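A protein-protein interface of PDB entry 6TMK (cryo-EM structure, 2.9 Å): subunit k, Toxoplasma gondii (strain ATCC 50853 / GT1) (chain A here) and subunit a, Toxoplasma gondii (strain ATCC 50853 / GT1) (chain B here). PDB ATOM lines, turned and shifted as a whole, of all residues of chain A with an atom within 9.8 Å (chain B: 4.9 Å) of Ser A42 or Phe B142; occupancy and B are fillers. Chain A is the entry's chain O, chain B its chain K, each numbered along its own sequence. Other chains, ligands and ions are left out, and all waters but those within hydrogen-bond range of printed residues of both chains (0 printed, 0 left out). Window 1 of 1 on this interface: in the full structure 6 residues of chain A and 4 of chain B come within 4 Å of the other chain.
SD of Met B139 lies close to O of Ser A41 (3.6 Å).
The backbone NH of Phe A51 sits at hydrogen-bond distance from the backbone carbonyl oxygen of Val A46.
Among the printed residues, merely in contact across the chains: Ser A42 with Lys B138, Ser A42 with Met B139, Ser A42 with Phe B142, Thr A43 with Phe B142, Val A46 with Met B139, Val A46 with Phe B142, Met A47 with Phe B142, Met A47 with Phe B146 and Phe A51 with Phe B146.
Of chain A, only Ser A42 (3.8 Å), Thr A43 (3.8 Å), Val A46 (3.7 Å) and Met A47 (3.9 Å) come within 4 Å of Phe B142.
Of chain A, only Ser A41 (3.6 Å), Ser A42 (3.6 Å) and Val A46 (3.9 Å) come within 4 Å of Met B139.
No residue of chain A comes within 4 Å of Ala B140.
No residue of chain A comes within 4 Å of Ala B143.
No residue of chain A comes within 4 Å of Ala B144.
No residue of chain A comes within 4 Å of Thr B145.
Of the printed residues of chain B, Met A47 touches Phe B142 (3.9 Å) and Phe B146 (3.8 Å).
Of the printed residues of chain B, Ser A41 touches Met B139 (3.6 Å).
Printed residues of chain B within 4 Å of Thr A43: Phe B142 (3.8 Å).
Of the printed residues of chain B, Phe A51 touches Phe B146.
Of the printed residues of chain B, Val A46 touches Met B139 and Phe B142.
Val A48 touches none of the printed residues of chain B.
Printed residues of chain B that touch a printed residue of chain A: Lys B138, Met B139, Phe B142 and Phe B146.
Of the 16 printed residues of chain A, 6 touch a printed residue of chain B.
Printed residues of chain A that touch a printed residue of chain B: Ser A41, Ser A42, Thr A43, Val A46, Met A47 and Phe A51.
Among the printed residues, 10 pairs touch across the chains.
Among the printed residues, no Asp or Glu carboxylate lies within 4 Å of a Lys or Arg side-chain nitrogen of the other chain.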
ATOM      1  N   PHE A  36       6.073  10.814 -23.194  1.00  0.00           N
ATOM      2  CA  PHE A  36       5.807   9.602 -23.956  1.00  0.00           C
ATOM      3  C   PHE A  36       6.846   9.404 -25.049  1.00  0.00           C
ATOM      4  O   PHE A  36       7.265   8.274 -25.318  1.00  0.00           O
ATOM      5  CB  PHE A  36       4.406   9.659 -24.554  1.00  0.00           C
ATOM      6  CG  PHE A  36       4.024   8.431 -25.318  1.00  0.00           C
ATOM      7  CD1 PHE A  36       3.522   7.326 -24.667  1.00  0.00           C
ATOM      8  CD2 PHE A  36       4.162   8.384 -26.690  1.00  0.00           C
ATOM      9  CE1 PHE A  36       3.174   6.199 -25.368  1.00  0.00           C
ATOM     10  CE2 PHE A  36       3.815   7.259 -27.390  1.00  0.00           C
ATOM     11  CZ  PHE A  36       3.320   6.167 -26.730  1.00  0.00           C
ATOM     12  N   TYR A  37       7.273  10.492 -25.687  1.00  0.00           N
ATOM     13  CA  TYR A  37       8.312  10.395 -26.700  1.00  0.00           C
ATOM     14  C   TYR A  37       9.611   9.892 -26.093  1.00  0.00           C
ATOM     15  O   TYR A  37      10.225   8.949 -26.605  1.00  0.00           O
ATOM     16  CB  TYR A  37       8.514  11.749 -27.368  1.00  0.00           C
ATOM     17  CG  TYR A  37       9.466  11.719 -28.535  1.00  0.00           C
ATOM     18  CD1 TYR A  37       9.012  11.462 -29.814  1.00  0.00           C
ATOM     19  CD2 TYR A  37      10.817  11.946 -28.358  1.00  0.00           C
ATOM     20  CE1 TYR A  37       9.873  11.432 -30.878  1.00  0.00           C
ATOM     21  CE2 TYR A  37      11.684  11.917 -29.417  1.00  0.00           C
ATOM     22  CZ  TYR A  37      11.209  11.659 -30.675  1.00  0.00           C
ATOM     23  OH  TYR A  37      12.082  11.632 -31.734  1.00  0.00           O
ATOM     24  N   SER A  39      10.670   7.830 -23.856  1.00  0.00           N
ATOM     25  CA  SER A  39      10.328   6.669 -23.055  1.00  0.00           C
ATOM     26  C   SER A  39      10.646   5.421 -23.858  1.00  0.00           C
ATOM     27  O   SER A  39      10.900   5.478 -25.062  1.00  0.00           O
ATOM     28  CB  SER A  39       8.864   6.688 -22.626  1.00  0.00           C
ATOM     29  OG  SER A  39       8.603   7.791 -21.784  1.00  0.00           O
ATOM     30  N   GLN A  40      10.627   4.284 -23.174  1.00  0.00           N
ATOM     31  CA  GLN A  40      10.959   3.017 -23.799  1.00  0.00           C
ATOM     32  C   GLN A  40       9.815   2.549 -24.685  1.00  0.00           C
ATOM     33  O   GLN A  40       8.654   2.543 -24.266  1.00  0.00           O
ATOM     34  CB  GLN A  40      11.249   1.971 -22.733  1.00  0.00           C
ATOM     35  CG  GLN A  40      12.551   2.151 -22.022  1.00  0.00           C
ATOM     36  CD  GLN A  40      13.070   0.862 -21.444  1.00  0.00           C
ATOM     37  OE1 GLN A  40      13.629   0.027 -22.153  1.00  0.00           O
ATOM     38  NE2 GLN A  40      12.887   0.689 -20.148  1.00  0.00           N
ATOM     39  N   SER A  41      10.150   2.147 -25.911  1.00  0.00           N
ATOM     40  CA  SER A  41       9.154   1.573 -26.805  1.00  0.00           C
ATOM     41  C   SER A  41       8.625   0.249 -26.276  1.00  0.00           C
ATOM     42  O   SER A  41       7.479  -0.116 -26.555  1.00  0.00           O
ATOM     43  CB  SER A  41       9.753   1.391 -28.194  1.00  0.00           C
ATOM     44  OG  SER A  41      10.082   2.642 -28.766  1.00  0.00           O
ATOM     45  N   SER A  42       9.438  -0.475 -25.509  1.00  0.00           N
ATOM     46  CA  SER A  42       9.047  -1.799 -25.049  1.00  0.00           C
ATOM     47  C   SER A  42       7.854  -1.740 -24.107  1.00  0.00           C
ATOM     48  O   SER A  42       7.014  -2.646 -24.118  1.00  0.00           O
ATOM     49  CB  SER A  42      10.228  -2.469 -24.356  1.00  0.00           C
ATOM     50  OG  SER A  42      11.294  -2.677 -25.261  1.00  0.00           O
ATOM     51  N   THR A  43       7.760  -0.695 -23.291  1.00  0.00           N
ATOM     52  CA  THR A  43       6.829  -0.647 -22.174  1.00  0.00           C
ATOM     53  C   THR A  43       5.677   0.317 -22.387  1.00  0.00           C
ATOM     54  O   THR A  43       4.555   0.037 -21.951  1.00  0.00           O
ATOM     55  CB  THR A  43       7.570  -0.237 -20.898  1.00  0.00           C
ATOM     56  OG1 THR A  43       7.929   1.144 -20.982  1.00  0.00           O
ATOM     57  CG2 THR A  43       8.825  -1.058 -20.713  1.00  0.00           C
ATOM     58  N   LYS A  44       5.935   1.454 -23.031  1.00  0.00           N
ATOM     59  CA  LYS A  44       4.976   2.549 -22.997  1.00  0.00           C
ATOM     60  C   LYS A  44       3.735   2.227 -23.815  1.00  0.00           C
ATOM     61  O   LYS A  44       2.615   2.514 -23.386  1.00  0.00           O
ATOM     62  CB  LYS A  44       5.643   3.828 -23.491  1.00  0.00           C
ATOM     63  CG  LYS A  44       5.938   3.852 -24.958  1.00  0.00           C
ATOM     64  CD  LYS A  44       6.895   4.957 -25.286  1.00  0.00           C
ATOM     65  CE  LYS A  44       7.129   5.070 -26.758  1.00  0.00           C
ATOM     66  NZ  LYS A  44       8.238   5.990 -27.035  1.00  0.00           N
ATOM     67  N   TYR A  45       3.909   1.621 -24.989  1.00  0.00           N
ATOM     68  CA  TYR A  45       2.756   1.317 -25.828  1.00  0.00           C
ATOM     69  C   TYR A  45       1.826   0.346 -25.124  1.00  0.00           C
ATOM     70  O   TYR A  45       0.612   0.564 -25.051  1.00  0.00           O
ATOM     71  CB  TYR A  45       3.218   0.750 -27.167  1.00  0.00           C
ATOM     72  CG  TYR A  45       3.952   1.748 -28.020  1.00  0.00           C
ATOM     73  CD1 TYR A  45       3.283   2.802 -28.613  1.00  0.00           C
ATOM     74  CD2 TYR A  45       5.313   1.638 -28.234  1.00  0.00           C
ATOM     75  CE1 TYR A  45       3.946   3.715 -29.393  1.00  0.00           C
ATOM     76  CE2 TYR A  45       5.985   2.548 -29.011  1.00  0.00           C
ATOM     77  CZ  TYR A  45       5.298   3.584 -29.588  1.00  0.00           C
ATOM     78  OH  TYR A  45       5.972   4.493 -30.366  1.00  0.00           O
ATOM     79  N   VAL A  46       2.394  -0.719 -24.562  1.00  0.00           N
ATOM     80  CA  VAL A  46       1.608  -1.659 -23.775  1.00  0.00           C
ATOM     81  C   VAL A  46       0.877  -0.923 -22.665  1.00  0.00           C
ATOM     82  O   VAL A  46      -0.357  -0.839 -22.662  1.00  0.00           O
ATOM     83  CB  VAL A  46       2.512  -2.766 -23.208  1.00  0.00           C
ATOM     84  CG1 VAL A  46       1.764  -3.600 -22.201  1.00  0.00           C
ATOM     85  CG2 VAL A  46       3.045  -3.630 -24.321  1.00  0.00           C
ATOM     86  N   MET A  47       1.637  -0.313 -21.754  1.00  0.00           N
ATOM     87  CA  MET A  47       1.069   0.253 -20.539  1.00  0.00           C
ATOM     88  C   MET A  47       0.086   1.382 -20.810  1.00  0.00           C
ATOM     89  O   MET A  47      -0.734   1.690 -19.941  1.00  0.00           O
ATOM     90  CB  MET A  47       2.197   0.759 -19.645  1.00  0.00           C
ATOM     91  CG  MET A  47       1.755   1.212 -18.272  1.00  0.00           C
ATOM     92  SD  MET A  47       1.013  -0.112 -17.308  1.00  0.00           S
ATOM     93  CE  MET A  47       2.477  -1.073 -16.966  1.00  0.00           C
ATOM     94  N   VAL A  48       0.147   2.010 -21.982  1.00  0.00           N
ATOM     95  CA  VAL A  48      -0.691   3.165 -22.266  1.00  0.00           C
ATOM     96  C   VAL A  48      -1.881   2.837 -23.161  1.00  0.00           C
ATOM     97  O   VAL A  48      -2.876   3.577 -23.134  1.00  0.00           O
ATOM     98  CB  VAL A  48       0.147   4.299 -22.888  1.00  0.00           C
ATOM     99  CG1 VAL A  48      -0.739   5.449 -23.316  1.00  0.00           C
ATOM    100  CG2 VAL A  48       1.172   4.787 -21.892  1.00  0.00           C
ATOM    101  N   PHE A  49      -1.819   1.762 -23.941  1.00  0.00           N
ATOM    102  CA  PHE A  49      -2.893   1.449 -24.872  1.00  0.00           C
ATOM    103  C   PHE A  49      -3.508   0.076 -24.672  1.00  0.00           C
ATOM    104  O   PHE A  49      -4.732  -0.053 -24.741  1.00  0.00           O
ATOM    105  CB  PHE A  49      -2.372   1.572 -26.305  1.00  0.00           C
ATOM    106  CG  PHE A  49      -2.015   2.973 -26.689  1.00  0.00           C
ATOM    107  CD1 PHE A  49      -2.998   3.927 -26.870  1.00  0.00           C
ATOM    108  CD2 PHE A  49      -0.698   3.340 -26.855  1.00  0.00           C
ATOM    109  CE1 PHE A  49      -2.670   5.217 -27.216  1.00  0.00           C
ATOM    110  CE2 PHE A  49      -0.364   4.628 -27.203  1.00  0.00           C
ATOM    111  CZ  PHE A  49      -1.351   5.568 -27.382  1.00  0.00           C
ATOM    112  N   LEU A  50      -2.709  -0.959 -24.423  1.00  0.00           N
ATOM    113  CA  LEU A  50      -3.244  -2.313 -24.477  1.00  0.00           C
ATOM    114  C   LEU A  50      -3.833  -2.753 -23.149  1.00  0.00           C
ATOM    115  O   LEU A  50      -4.858  -3.441 -23.127  1.00  0.00           O
ATOM    116  CB  LEU A  50      -2.153  -3.289 -24.915  1.00  0.00           C
ATOM    117  CG  LEU A  50      -1.379  -2.881 -26.167  1.00  0.00           C
ATOM    118  CD1 LEU A  50      -0.453  -3.995 -26.590  1.00  0.00           C
ATOM    119  CD2 LEU A  50      -2.320  -2.509 -27.294  1.00  0.00           C
ATOM    120  N   PHE A  51      -3.207  -2.373 -22.038  1.00  0.00           N
ATOM    121  CA  PHE A  51      -3.808  -2.663 -20.740  1.00  0.00           C
ATOM    122  C   PHE A  51      -5.006  -1.766 -20.477  1.00  0.00           C
ATOM    123  O   PHE A  51      -6.064  -2.281 -20.072  1.00  0.00           O
ATOM    124  CB  PHE A  51      -2.751  -2.531 -19.641  1.00  0.00           C
ATOM    125  CG  PHE A  51      -1.754  -3.654 -19.608  1.00  0.00           C
ATOM    126  CD1 PHE A  51      -1.949  -4.816 -20.332  1.00  0.00           C
ATOM    127  CD2 PHE A  51      -0.615  -3.544 -18.837  1.00  0.00           C
ATOM    128  CE1 PHE A  51      -1.032  -5.833 -20.287  1.00  0.00           C
ATOM    129  CE2 PHE A  51       0.303  -4.559 -18.792  1.00  0.00           C
ATOM    130  CZ  PHE A  51       0.093  -5.705 -19.516  1.00  0.00           C
ATOM    131  N   PRO A  52      -4.928  -0.451 -20.674  1.00  0.00           N
ATOM    132  CA  PRO A  52      -6.140   0.371 -20.596  1.00  0.00           C
ATOM    133  C   PRO A  52      -7.265  -0.111 -21.488  1.00  0.00           C
ATOM    134  O   PRO A  52      -8.415  -0.145 -21.046  1.00  0.00           O
ATOM    135  CB  PRO A  52      -5.630   1.749 -21.026  1.00  0.00           C
ATOM    136  CG  PRO A  52      -4.235   1.776 -20.570  1.00  0.00           C
ATOM    137  CD  PRO A  52      -3.712   0.374 -20.668  1.00  0.00           C
ATOM    138  N   LYS B 138       9.665  -8.183 -27.474  1.00  0.00           N
ATOM    139  CA  LYS B 138      10.089  -7.510 -26.252  1.00  0.00           C
ATOM    140  C   LYS B 138       8.893  -6.962 -25.490  1.00  0.00           C
ATOM    141  O   LYS B 138       8.861  -7.008 -24.255  1.00  0.00           O
ATOM    142  CB  LYS B 138      11.068  -6.389 -26.582  1.00  0.00           C
ATOM    143  CG  LYS B 138      12.371  -6.874 -27.158  1.00  0.00           C
ATOM    144  CD  LYS B 138      13.313  -7.336 -26.072  1.00  0.00           C
ATOM    145  CE  LYS B 138      14.650  -7.767 -26.644  1.00  0.00           C
ATOM    146  NZ  LYS B 138      15.472  -8.488 -25.639  1.00  0.00           N
ATOM    147  N   MET B 139       7.898  -6.442 -26.208  1.00  0.00           N
ATOM    148  CA  MET B 139       6.697  -5.955 -25.538  1.00  0.00           C
ATOM    149  C   MET B 139       5.977  -7.088 -24.815  1.00  0.00           C
ATOM    150  O   MET B 139       5.524  -6.926 -23.673  1.00  0.00           O
ATOM    151  CB  MET B 139       5.772  -5.292 -26.554  1.00  0.00           C
ATOM    152  CG  MET B 139       6.407  -4.138 -27.293  1.00  0.00           C
ATOM    153  SD  MET B 139       5.282  -2.761 -27.562  1.00  0.00           S
ATOM    154  CE  MET B 139       4.001  -3.569 -28.508  1.00  0.00           C
ATOM    155  N   ALA B 140       5.868  -8.247 -25.464  1.00  0.00           N
ATOM    156  CA  ALA B 140       5.235  -9.403 -24.839  1.00  0.00           C
ATOM    157  C   ALA B 140       6.032  -9.886 -23.637  1.00  0.00           C
ATOM    158  O   ALA B 140       5.454 -10.257 -22.608  1.00  0.00           O
ATOM    159  CB  ALA B 140       5.083 -10.524 -25.859  1.00  0.00           C
ATOM    160  N   SER B 141       7.361  -9.907 -23.750  1.00  0.00           N
ATOM    161  CA  SER B 141       8.189 -10.296 -22.615  1.00  0.00           C
ATOM    162  C   SER B 141       7.988  -9.345 -21.445  1.00  0.00           C
ATOM    163  O   SER B 141       7.910  -9.777 -20.288  1.00  0.00           O
ATOM    164  CB  SER B 141       9.655 -10.337 -23.030  1.00  0.00           C
ATOM    165  OG  SER B 141      10.485 -10.674 -21.936  1.00  0.00           O
ATOM    166  N   PHE B 142       7.894  -8.046 -21.727  1.00  0.00           N
ATOM    167  CA  PHE B 142       7.653  -7.079 -20.666  1.00  0.00           C
ATOM    168  C   PHE B 142       6.309  -7.328 -20.003  1.00  0.00           C
ATOM    169  O   PHE B 142       6.201  -7.314 -18.774  1.00  0.00           O
ATOM    170  CB  PHE B 142       7.708  -5.656 -21.213  1.00  0.00           C
ATOM    171  CG  PHE B 142       6.870  -4.694 -20.436  1.00  0.00           C
ATOM    172  CD1 PHE B 142       7.268  -4.252 -19.193  1.00  0.00           C
ATOM    173  CD2 PHE B 142       5.670  -4.247 -20.943  1.00  0.00           C
ATOM    174  CE1 PHE B 142       6.488  -3.379 -18.478  1.00  0.00           C
ATOM    175  CE2 PHE B 142       4.889  -3.377 -20.231  1.00  0.00           C
ATOM    176  CZ  PHE B 142       5.298  -2.941 -18.997  1.00  0.00           C
ATOM    177  N   ALA B 143       5.264  -7.527 -20.804  1.00  0.00           N
ATOM    178  CA  ALA B 143       3.944  -7.776 -20.236  1.00  0.00           C
ATOM    179  C   ALA B 143       3.950  -9.021 -19.363  1.00  0.00           C
ATOM    180  O   ALA B 143       3.392  -9.022 -18.258  1.00  0.00           O
ATOM    181  CB  ALA B 143       2.915  -7.914 -21.349  1.00  0.00           C
ATOM    182  N   ALA B 144       4.579 -10.093 -19.843  1.00  0.00           N
ATOM    183  CA  ALA B 144       4.643 -11.326 -19.071  1.00  0.00           C
ATOM    184  C   ALA B 144       5.365 -11.107 -17.751  1.00  0.00           C
ATOM    185  O   ALA B 144       4.878 -11.512 -16.692  1.00  0.00           O
ATOM    186  CB  ALA B 144       5.335 -12.409 -19.890  1.00  0.00           C
ATOM    187  N   THR B 145       6.542 -10.481 -17.797  1.00  0.00           N
ATOM    188  CA  THR B 145       7.302 -10.246 -16.574  1.00  0.00           C
ATOM    189  C   THR B 145       6.520  -9.367 -15.607  1.00  0.00           C
ATOM    190  O   THR B 145       6.509  -9.613 -14.394  1.00  0.00           O
ATOM    191  CB  THR B 145       8.646  -9.604 -16.918  1.00  0.00           C
ATOM    192  OG1 THR B 145       9.251 -10.309 -18.006  1.00  0.00           O
ATOM    193  CG2 THR B 145       9.573  -9.641 -15.731  1.00  0.00           C
ATOM    194  N   PHE B 146       5.845  -8.346 -16.131  1.00  0.00           N
ATOM    195  CA  PHE B 146       5.095  -7.425 -15.291  1.00  0.00           C
ATOM    196  C   PHE B 146       3.943  -8.127 -14.592  1.00  0.00           C
ATOM    197  O   PHE B 146       3.702  -7.904 -13.401  1.00  0.00           O
ATOM    198  CB  PHE B 146       4.589  -6.260 -16.137  1.00  0.00           C
ATOM    199  CG  PHE B 146       3.749  -5.283 -15.382  1.00  0.00           C
ATOM    200  CD1 PHE B 146       4.330  -4.325 -14.581  1.00  0.00           C
ATOM    201  CD2 PHE B 146       2.375  -5.319 -15.481  1.00  0.00           C
ATOM    202  CE1 PHE B 146       3.556  -3.427 -13.891  1.00  0.00           C
ATOM    203  CE2 PHE B 146       1.599  -4.425 -14.793  1.00  0.00           C
ATOM    204  CZ  PHE B 146       2.188  -3.478 -13.996  1.00  0.00           C
ATOM    205  N   LEU B 147       3.219  -8.983 -15.314  1.00  0.00           N
ATOM    206  CA  LEU B 147       2.130  -9.718 -14.682  1.00  0.00           C
ATOM    207  C   LEU B 147       2.659 -10.755 -13.699  1.00  0.00           C
ATOM    208  O   LEU B 147       2.062 -10.969 -12.639  1.00  0.00           O
ATOM    209  CB  LEU B 147       1.266 -10.381 -15.749  1.00  0.00           C
ATOM    210  CG  LEU B 147       0.579  -9.423 -16.718  1.00  0.00           C
ATOM    211  CD1 LEU B 147       0.002 -10.181 -17.890  1.00  0.00           C
ATOM    212  CD2 LEU B 147      -0.493  -8.626 -16.023  1.00  0.00           C
